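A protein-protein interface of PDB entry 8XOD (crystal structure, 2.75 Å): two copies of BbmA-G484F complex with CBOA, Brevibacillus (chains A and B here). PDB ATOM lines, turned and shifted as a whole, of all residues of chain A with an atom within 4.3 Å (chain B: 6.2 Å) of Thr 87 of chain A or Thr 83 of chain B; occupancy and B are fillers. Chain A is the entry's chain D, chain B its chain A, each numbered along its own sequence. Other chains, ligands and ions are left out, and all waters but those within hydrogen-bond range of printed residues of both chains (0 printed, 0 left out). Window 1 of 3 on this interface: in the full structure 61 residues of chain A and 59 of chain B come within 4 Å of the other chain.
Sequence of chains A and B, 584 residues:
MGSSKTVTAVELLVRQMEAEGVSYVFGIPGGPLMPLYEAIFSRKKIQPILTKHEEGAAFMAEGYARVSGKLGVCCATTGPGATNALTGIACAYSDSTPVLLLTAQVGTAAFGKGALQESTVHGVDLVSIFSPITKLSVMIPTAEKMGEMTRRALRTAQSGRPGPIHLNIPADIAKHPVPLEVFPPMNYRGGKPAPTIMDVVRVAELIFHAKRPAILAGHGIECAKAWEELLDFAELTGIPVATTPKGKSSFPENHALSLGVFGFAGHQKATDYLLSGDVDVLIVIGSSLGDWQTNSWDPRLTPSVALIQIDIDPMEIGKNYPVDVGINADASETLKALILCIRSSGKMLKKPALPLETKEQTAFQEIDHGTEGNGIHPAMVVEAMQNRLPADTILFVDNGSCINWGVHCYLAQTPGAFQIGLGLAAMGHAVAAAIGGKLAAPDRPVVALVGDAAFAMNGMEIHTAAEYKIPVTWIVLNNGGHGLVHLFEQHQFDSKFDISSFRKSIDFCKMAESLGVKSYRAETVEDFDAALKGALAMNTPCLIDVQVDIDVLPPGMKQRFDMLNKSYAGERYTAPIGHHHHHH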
ATOM      1  N   GLU A  55      19.348   0.013 -18.965  1.00  0.00           N
ATOM      2  CA  GLU A  55      18.026   0.019 -19.591  1.00  0.00           C
ATOM      3  C   GLU A  55      16.941   0.115 -18.543  1.00  0.00           C
ATOM      4  O   GLU A  55      15.869   0.678 -18.804  1.00  0.00           O
ATOM      5  CB  GLU A  55      17.818  -1.189 -20.490  1.00  0.00           C
ATOM      6  CG  GLU A  55      17.582  -2.482 -19.809  1.00  0.00           C
ATOM      7  CD  GLU A  55      16.942  -3.463 -20.759  1.00  0.00           C
ATOM      8  OE1 GLU A  55      16.252  -2.991 -21.696  1.00  0.00           O
ATOM      9  OE2 GLU A  55      17.132  -4.687 -20.581  1.00  0.00           O
ATOM     10  N   ASN A  84      23.758   0.421 -23.192  1.00  0.00           N
ATOM     11  CA  ASN A  84      22.810  -0.354 -22.404  1.00  0.00           C
ATOM     12  C   ASN A  84      21.445   0.309 -22.367  1.00  0.00           C
ATOM     13  O   ASN A  84      20.412  -0.370 -22.448  1.00  0.00           O
ATOM     14  CB  ASN A  84      23.339  -0.547 -20.988  1.00  0.00           C
ATOM     15  CG  ASN A  84      23.782  -1.946 -20.743  1.00  0.00           C
ATOM     16  OD1 ASN A  84      23.611  -2.807 -21.607  1.00  0.00           O
ATOM     17  ND2 ASN A  84      24.325  -2.202 -19.559  1.00  0.00           N
ATOM     18  N   ALA A  85      21.420   1.635 -22.274  1.00  0.00           N
ATOM     19  CA  ALA A  85      20.146   2.321 -22.133  1.00  0.00           C
ATOM     20  C   ALA A  85      19.325   2.331 -23.410  1.00  0.00           C
ATOM     21  O   ALA A  85      18.115   2.572 -23.341  1.00  0.00           O
ATOM     22  CB  ALA A  85      20.389   3.759 -21.675  1.00  0.00           C
ATOM     23  N   LEU A  86      19.923   1.961 -24.544  1.00  0.00           N
ATOM     24  CA  LEU A  86      19.304   2.255 -25.837  1.00  0.00           C
ATOM     25  C   LEU A  86      17.869   1.747 -25.921  1.00  0.00           C
ATOM     26  O   LEU A  86      16.986   2.430 -26.442  1.00  0.00           O
ATOM     27  CB  LEU A  86      20.138   1.692 -26.987  1.00  0.00           C
ATOM     28  CG  LEU A  86      19.553   2.174 -28.320  1.00  0.00           C
ATOM     29  CD1 LEU A  86      20.587   2.851 -29.208  1.00  0.00           C
ATOM     30  CD2 LEU A  86      18.835   1.031 -29.047  1.00  0.00           C
ATOM     31  N   THR A  87      17.620   0.533 -25.461  1.00  0.00           N
ATOM     32  CA  THR A  87      16.299  -0.016 -25.691  1.00  0.00           C
ATOM     33  C   THR A  87      15.233   0.802 -24.972  1.00  0.00           C
ATOM     34  O   THR A  87      14.103   0.911 -25.463  1.00  0.00           O
ATOM     35  CB  THR A  87      16.250  -1.474 -25.219  1.00  0.00           C
ATOM     36  OG1 THR A  87      17.315  -2.232 -25.829  1.00  0.00           O
ATOM     37  CG2 THR A  87      14.873  -2.096 -25.522  1.00  0.00           C
ATOM     38  N   GLY A  88      15.588   1.415 -23.837  1.00  0.00           N
ATOM     39  CA  GLY A  88      14.649   2.274 -23.139  1.00  0.00           C
ATOM     40  C   GLY A  88      14.434   3.584 -23.864  1.00  0.00           C
ATOM     41  O   GLY A  88      13.309   4.088 -23.940  1.00  0.00           O
ATOM     42  N   ILE A  89      15.508   4.133 -24.437  1.00  0.00           N
ATOM     43  CA  ILE A  89      15.398   5.341 -25.224  1.00  0.00           C
ATOM     44  C   ILE A  89      14.596   5.073 -26.480  1.00  0.00           C
ATOM     45  O   ILE A  89      13.923   5.972 -26.997  1.00  0.00           O
ATOM     46  CB  ILE A  89      16.798   5.883 -25.551  1.00  0.00           C
ATOM     47  CG1 ILE A  89      17.628   5.976 -24.270  1.00  0.00           C
ATOM     48  CG2 ILE A  89      16.703   7.214 -26.278  1.00  0.00           C
ATOM     49  CD1 ILE A  89      16.894   6.620 -23.124  1.00  0.00           C
ATOM     50  N   ALA A  90      14.680   3.851 -27.015  1.00  0.00           N
ATOM     51  CA  ALA A  90      13.896   3.499 -28.195  1.00  0.00           C
ATOM     52  C   ALA A  90      12.416   3.358 -27.861  1.00  0.00           C
ATOM     53  O   ALA A  90      11.563   3.565 -28.734  1.00  0.00           O
ATOM     54  CB  ALA A  90      14.438   2.216 -28.837  1.00  0.00           C
ATOM     55  N   CYS A  91      12.086   3.014 -26.614  1.00  0.00           N
ATOM     56  CA  CYS A  91      10.681   2.946 -26.229  1.00  0.00           C
ATOM     57  C   CYS A  91      10.103   4.341 -25.982  1.00  0.00           C
ATOM     58  O   CYS A  91       9.004   4.658 -26.462  1.00  0.00           O
ATOM     59  CB  CYS A  91      10.540   2.079 -24.978  1.00  0.00           C
ATOM     60  SG  CYS A  91      10.806   0.295 -25.224  1.00  0.00           S
ATOM     61  N   HIS B  53      17.939 -12.734 -21.976  1.00  0.00           N
ATOM     62  CA  HIS B  53      18.039 -11.371 -22.454  1.00  0.00           C
ATOM     63  C   HIS B  53      18.879 -11.443 -23.713  1.00  0.00           C
ATOM     64  O   HIS B  53      19.812 -12.250 -23.780  1.00  0.00           O
ATOM     65  CB  HIS B  53      18.685 -10.473 -21.388  1.00  0.00           C
ATOM     66  CG  HIS B  53      18.502  -9.005 -21.618  1.00  0.00           C
ATOM     67  ND1 HIS B  53      19.041  -8.348 -22.702  1.00  0.00           N
ATOM     68  CD2 HIS B  53      17.863  -8.062 -20.887  1.00  0.00           C
ATOM     69  CE1 HIS B  53      18.733  -7.067 -22.635  1.00  0.00           C
ATOM     70  NE2 HIS B  53      18.016  -6.868 -21.544  1.00  0.00           N
ATOM     71  N   ALA B  76      17.739 -12.024 -32.844  1.00  0.00           N
ATOM     72  CA  ALA B  76      16.816 -11.232 -32.053  1.00  0.00           C
ATOM     73  C   ALA B  76      15.701 -10.770 -32.973  1.00  0.00           C
ATOM     74  O   ALA B  76      15.900 -10.661 -34.191  1.00  0.00           O
ATOM     75  CB  ALA B  76      17.509 -10.031 -31.393  1.00  0.00           C
ATOM     76  N   THR B  77      14.534 -10.481 -32.381  1.00  0.00           N
ATOM     77  CA  THR B  77      13.357 -10.111 -33.165  1.00  0.00           C
ATOM     78  C   THR B  77      13.385  -8.609 -33.504  1.00  0.00           C
ATOM     79  O   THR B  77      14.370  -7.895 -33.257  1.00  0.00           O
ATOM     80  CB  THR B  77      12.063 -10.493 -32.418  1.00  0.00           C
ATOM     81  OG1 THR B  77      10.938 -10.438 -33.305  1.00  0.00           O
ATOM     82  CG2 THR B  77      11.789  -9.539 -31.250  1.00  0.00           C
ATOM     83  N   GLY B  79      12.687  -4.632 -33.483  1.00  0.00           N
ATOM     84  CA  GLY B  79      12.606  -3.604 -32.476  1.00  0.00           C
ATOM     85  C   GLY B  79      13.387  -3.885 -31.210  1.00  0.00           C
ATOM     86  O   GLY B  79      14.622  -3.916 -31.214  1.00  0.00           O
ATOM     87  N   PRO B  80      12.681  -4.079 -30.087  1.00  0.00           N
ATOM     88  CA  PRO B  80      13.388  -4.170 -28.802  1.00  0.00           C
ATOM     89  C   PRO B  80      14.241  -5.419 -28.702  1.00  0.00           C
ATOM     90  O   PRO B  80      15.273  -5.411 -28.015  1.00  0.00           O
ATOM     91  CB  PRO B  80      12.245  -4.195 -27.784  1.00  0.00           C
ATOM     92  CG  PRO B  80      11.186  -4.988 -28.502  1.00  0.00           C
ATOM     93  CD  PRO B  80      11.277  -4.503 -29.958  1.00  0.00           C
ATOM     94  N   GLY B  81      13.847  -6.482 -29.407  1.00  0.00           N
ATOM     95  CA  GLY B  81      14.700  -7.651 -29.496  1.00  0.00           C
ATOM     96  C   GLY B  81      16.105  -7.316 -29.946  1.00  0.00           C
ATOM     97  O   GLY B  81      17.080  -7.685 -29.287  1.00  0.00           O
ATOM     98  N   ALA B  82      16.228  -6.598 -31.067  1.00  0.00           N
ATOM     99  CA  ALA B  82      17.551  -6.276 -31.600  1.00  0.00           C
ATOM    100  C   ALA B  82      18.273  -5.237 -30.736  1.00  0.00           C
ATOM    101  O   ALA B  82      19.443  -5.419 -30.385  1.00  0.00           O
ATOM    102  CB  ALA B  82      17.428  -5.818 -33.050  1.00  0.00           C
ATOM    103  N   THR B  83      17.587  -4.151 -30.354  1.00  0.00           N
ATOM    104  CA  THR B  83      18.234  -3.122 -29.535  1.00  0.00           C
ATOM    105  C   THR B  83      18.841  -3.699 -28.251  1.00  0.00           C
ATOM    106  O   THR B  83      19.869  -3.197 -27.776  1.00  0.00           O
ATOM    107  CB  THR B  83      17.237  -2.008 -29.175  1.00  0.00           C
ATOM    108  OG1 THR B  83      16.134  -2.551 -28.437  1.00  0.00           O
ATOM    109  CG2 THR B  83      16.702  -1.321 -30.418  1.00  0.00           C
ATOM    110  N   ASN B  84      18.242  -4.759 -27.681  1.00  0.00           N
ATOM    111  CA  ASN B  84      18.815  -5.352 -26.469  1.00  0.00           C
ATOM    112  C   ASN B  84      20.200  -5.929 -26.757  1.00  0.00           C
ATOM    113  O   ASN B  84      21.128  -5.803 -25.943  1.00  0.00           O
ATOM    114  CB  ASN B  84      17.891  -6.441 -25.918  1.00  0.00           C
ATOM    115  CG  ASN B  84      16.920  -5.916 -24.863  1.00  0.00           C
ATOM    116  OD1 ASN B  84      16.938  -4.731 -24.524  1.00  0.00           O
ATOM    117  ND2 ASN B  84      16.069  -6.802 -24.337  1.00  0.00           N
ATOM    118  N   ALA B  85      20.370  -6.521 -27.938  1.00  0.00           N
ATOM    119  CA  ALA B  85      21.626  -7.138 -28.302  1.00  0.00           C
ATOM    120  C   ALA B  85      22.732  -6.120 -28.564  1.00  0.00           C
ATOM    121  O   ALA B  85      23.889  -6.516 -28.737  1.00  0.00           O
ATOM    122  CB  ALA B  85      21.403  -8.018 -29.531  1.00  0.00           C
ATOM    123  N   LEU B  86      22.413  -4.824 -28.597  1.00  0.00           N
ATOM    124  CA  LEU B  86      23.383  -3.847 -29.081  1.00  0.00           C
ATOM    125  C   LEU B  86      24.693  -3.905 -28.304  1.00  0.00           C
ATOM    126  O   LEU B  86      25.776  -3.877 -28.895  1.00  0.00           O
ATOM    127  CB  LEU B  86      22.805  -2.441 -29.039  1.00  0.00           C
ATOM    128  CG  LEU B  86      23.882  -1.527 -29.613  1.00  0.00           C
ATOM    129  CD1 LEU B  86      23.348  -0.868 -30.845  1.00  0.00           C
ATOM    130  CD2 LEU B  86      24.378  -0.512 -28.576  1.00  0.00           C
ATOM    131  N   THR B  87      24.622  -3.929 -26.975  1.00  0.00           N
ATOM    132  CA  THR B  87      25.848  -3.799 -26.206  1.00  0.00           C
ATOM    133  C   THR B  87      26.760  -5.002 -26.420  1.00  0.00           C
ATOM    134  O   THR B  87      27.991  -4.857 -26.438  1.00  0.00           O
ATOM    135  CB  THR B  87      25.514  -3.624 -24.721  1.00  0.00           C
ATOM    136  OG1 THR B  87      24.834  -2.377 -24.522  1.00  0.00           O
ATOM    137  CG2 THR B  87      26.787  -3.673 -23.844  1.00  0.00           C
ATOM    138  N   VAL B 124      11.901   2.114 -35.717  1.00  0.00           N
ATOM    139  CA  VAL B 124      13.159   1.961 -34.989  1.00  0.00           C
ATOM    140  C   VAL B 124      14.187   1.381 -35.966  1.00  0.00           C
ATOM    141  O   VAL B 124      14.179   0.178 -36.238  1.00  0.00           O
ATOM    142  CB  VAL B 124      12.984   1.073 -33.755  1.00  0.00           C
ATOM    143  CG1 VAL B 124      14.336   0.761 -33.124  1.00  0.00           C
ATOM    144  CG2 VAL B 124      12.074   1.741 -32.752  1.00  0.00           C
ATOM    145  N   LEU B 126      16.861  -0.386 -37.306  1.00  0.00           N
ATOM    146  CA  LEU B 126      17.864  -1.333 -36.839  1.00  0.00           C
ATOM    147  C   LEU B 126      19.149  -1.213 -37.640  1.00  0.00           C
ATOM    148  O   LEU B 126      20.237  -1.142 -37.055  1.00  0.00           O
ATOM    149  CB  LEU B 126      17.312  -2.758 -36.885  1.00  0.00           C
ATOM    150  CG  LEU B 126      16.114  -2.903 -35.940  1.00  0.00           C
ATOM    151  CD1 LEU B 126      15.575  -4.324 -35.909  1.00  0.00           C
ATOM    152  CD2 LEU B 126      16.504  -2.431 -34.548  1.00  0.00           C
ATOM    153  N   ILE B 129      20.995   2.019 -36.578  1.00  0.00           N
ATOM    154  CA  ILE B 129      21.483   1.968 -35.202  1.00  0.00           C
ATOM    155  C   ILE B 129      22.756   1.127 -35.116  1.00  0.00           C
ATOM    156  O   ILE B 129      23.726   1.493 -34.433  1.00  0.00           O
ATOM    157  CB  ILE B 129      20.393   1.403 -34.283  1.00  0.00           C
ATOM    158  CG1 ILE B 129      19.244   2.399 -34.166  1.00  0.00           C
ATOM    159  CG2 ILE B 129      20.976   1.059 -32.936  1.00  0.00           C
ATOM    160  CD1 ILE B 129      17.989   1.809 -33.525  1.00  0.00           C
ATOM    161  N   PHE B 130      22.788   0.014 -35.851  1.00  0.00           N
ATOM    162  CA  PHE B 130      23.857  -0.973 -35.775  1.00  0.00           C
ATOM    163  C   PHE B 130      25.014  -0.643 -36.702  1.00  0.00           C
ATOM    164  O   PHE B 130      26.004  -1.369 -36.728  1.00  0.00           O
ATOM    165  CB  PHE B 130      23.292  -2.373 -36.075  1.00  0.00           C
ATOM    166  CG  PHE B 130      22.714  -3.062 -34.859  1.00  0.00           C
ATOM    167  CD1 PHE B 130      23.541  -3.757 -33.988  1.00  0.00           C
ATOM    168  CD2 PHE B 130      21.367  -2.990 -34.571  1.00  0.00           C
ATOM    169  CE1 PHE B 130      23.052  -4.381 -32.853  1.00  0.00           C
ATOM    170  CE2 PHE B 130      20.843  -3.618 -33.409  1.00  0.00           C
ATOM    171  CZ  PHE B 130      21.692  -4.309 -32.549  1.00  0.00           C
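The side-chain carboxylate of Glu 55 of chain A sits at hydrogen-bond distance from a ring nitrogen (NE2) of His 53 of chain B (2.5 Å). OG1 of Thr 83 of chain B lies within hydrogen-bond range of OG1 of Thr 87 of chain A. The side-chain amide oxygen of Asn 84 of chain B sits close to the side-chain carboxylate of Glu 55 of chain A (3.4 Å). OG1 of Thr 87 of chain A sits at hydrogen-bond distance from OD1 of Asn 84 of chain B, 2.8 Å away. The side-chain hydroxyl (OG1) of Thr 87 of chain B sits at hydrogen-bond distance from the side-chain amide oxygen (OD1) of Asn 84 of chain A (3.2 Å).
The side-chain amide nitrogen (ND2) of Asn 84 of chain B lies close to a ring nitrogen (NE2) of His 53 of chain B, 3.4 Å away. O of Gly 79 of chain B lies close to OG1 of Thr 83 of chain B (3.4 Å). OG1 of Thr 83 of chain B is in hydrogen-bond range of O of Pro 80 of chain B (3.0 Å). The backbone carbonyl oxygen (O) of Thr 87 of chain A lies within hydrogen-bond range of the side-chain sulfur (SG) of Cys 91 of chain A, at 3.4 Å.
Thr 83 of chain B touches Leu 86 of chain A (CB to CD2, 3.4 Å).
Printed residues of chain B within 4 Å of Thr 87 of chain A: Thr 83 (2.9 Å) and Asn 84 (2.8 Å). Of chain A, only Leu 86 and Thr 87 come within 4 Å of Thr 83 of chain B. Printed residues of chain A within 4 Å of His 53 of chain B: Glu 55. Printed residues of chain B within 4 Å of Asn 84 of chain A: Thr 87. Of the printed residues of chain A, Thr 87 of chain B touches Asn 84. Of the printed residues of chain A, Asn 84 of chain B touches Glu 55 and Thr 87. Printed residues of chain B within 4 Å of Glu 55 of chain A: His 53 (2.5 Å) and Asn 84 (3.4 Å). Pro 80 of chain B touches none of the printed residues of chain A. The nearest printed residue of chain A that does not touch Thr 83 of chain B is Ala 90 of chain A (4.5 Å).
Printed residues of chain A that touch a printed residue of chain B: Glu 55, Asn 84, Leu 86 and Thr 87. Hydrophobic or aromatic side chains of chain A that line the printed part of chain B: Leu 86. Printed residues of chain B that touch a printed residue of chain A: His 53, Thr 83, Asn 84 and Thr 87. Along chain B the printed residues that touch a printed residue of chain A span positions 53 to 87. Among the printed residues, 6 pairs touch across the chains. Among the printed residues, no Asp or Glu carboxylate lies within 4 Å of a Lys or Arg side-chain nitrogen of the other chain.
Asn 84 of chain A touches Thr 87 of chain B, and with the chains exchanged Thr 87 of chain A touches Asn 84 of chain B. Of the 6 pairs that touch across the chains among the printed residues, 2 have their exchanged pair printed and touching as well.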
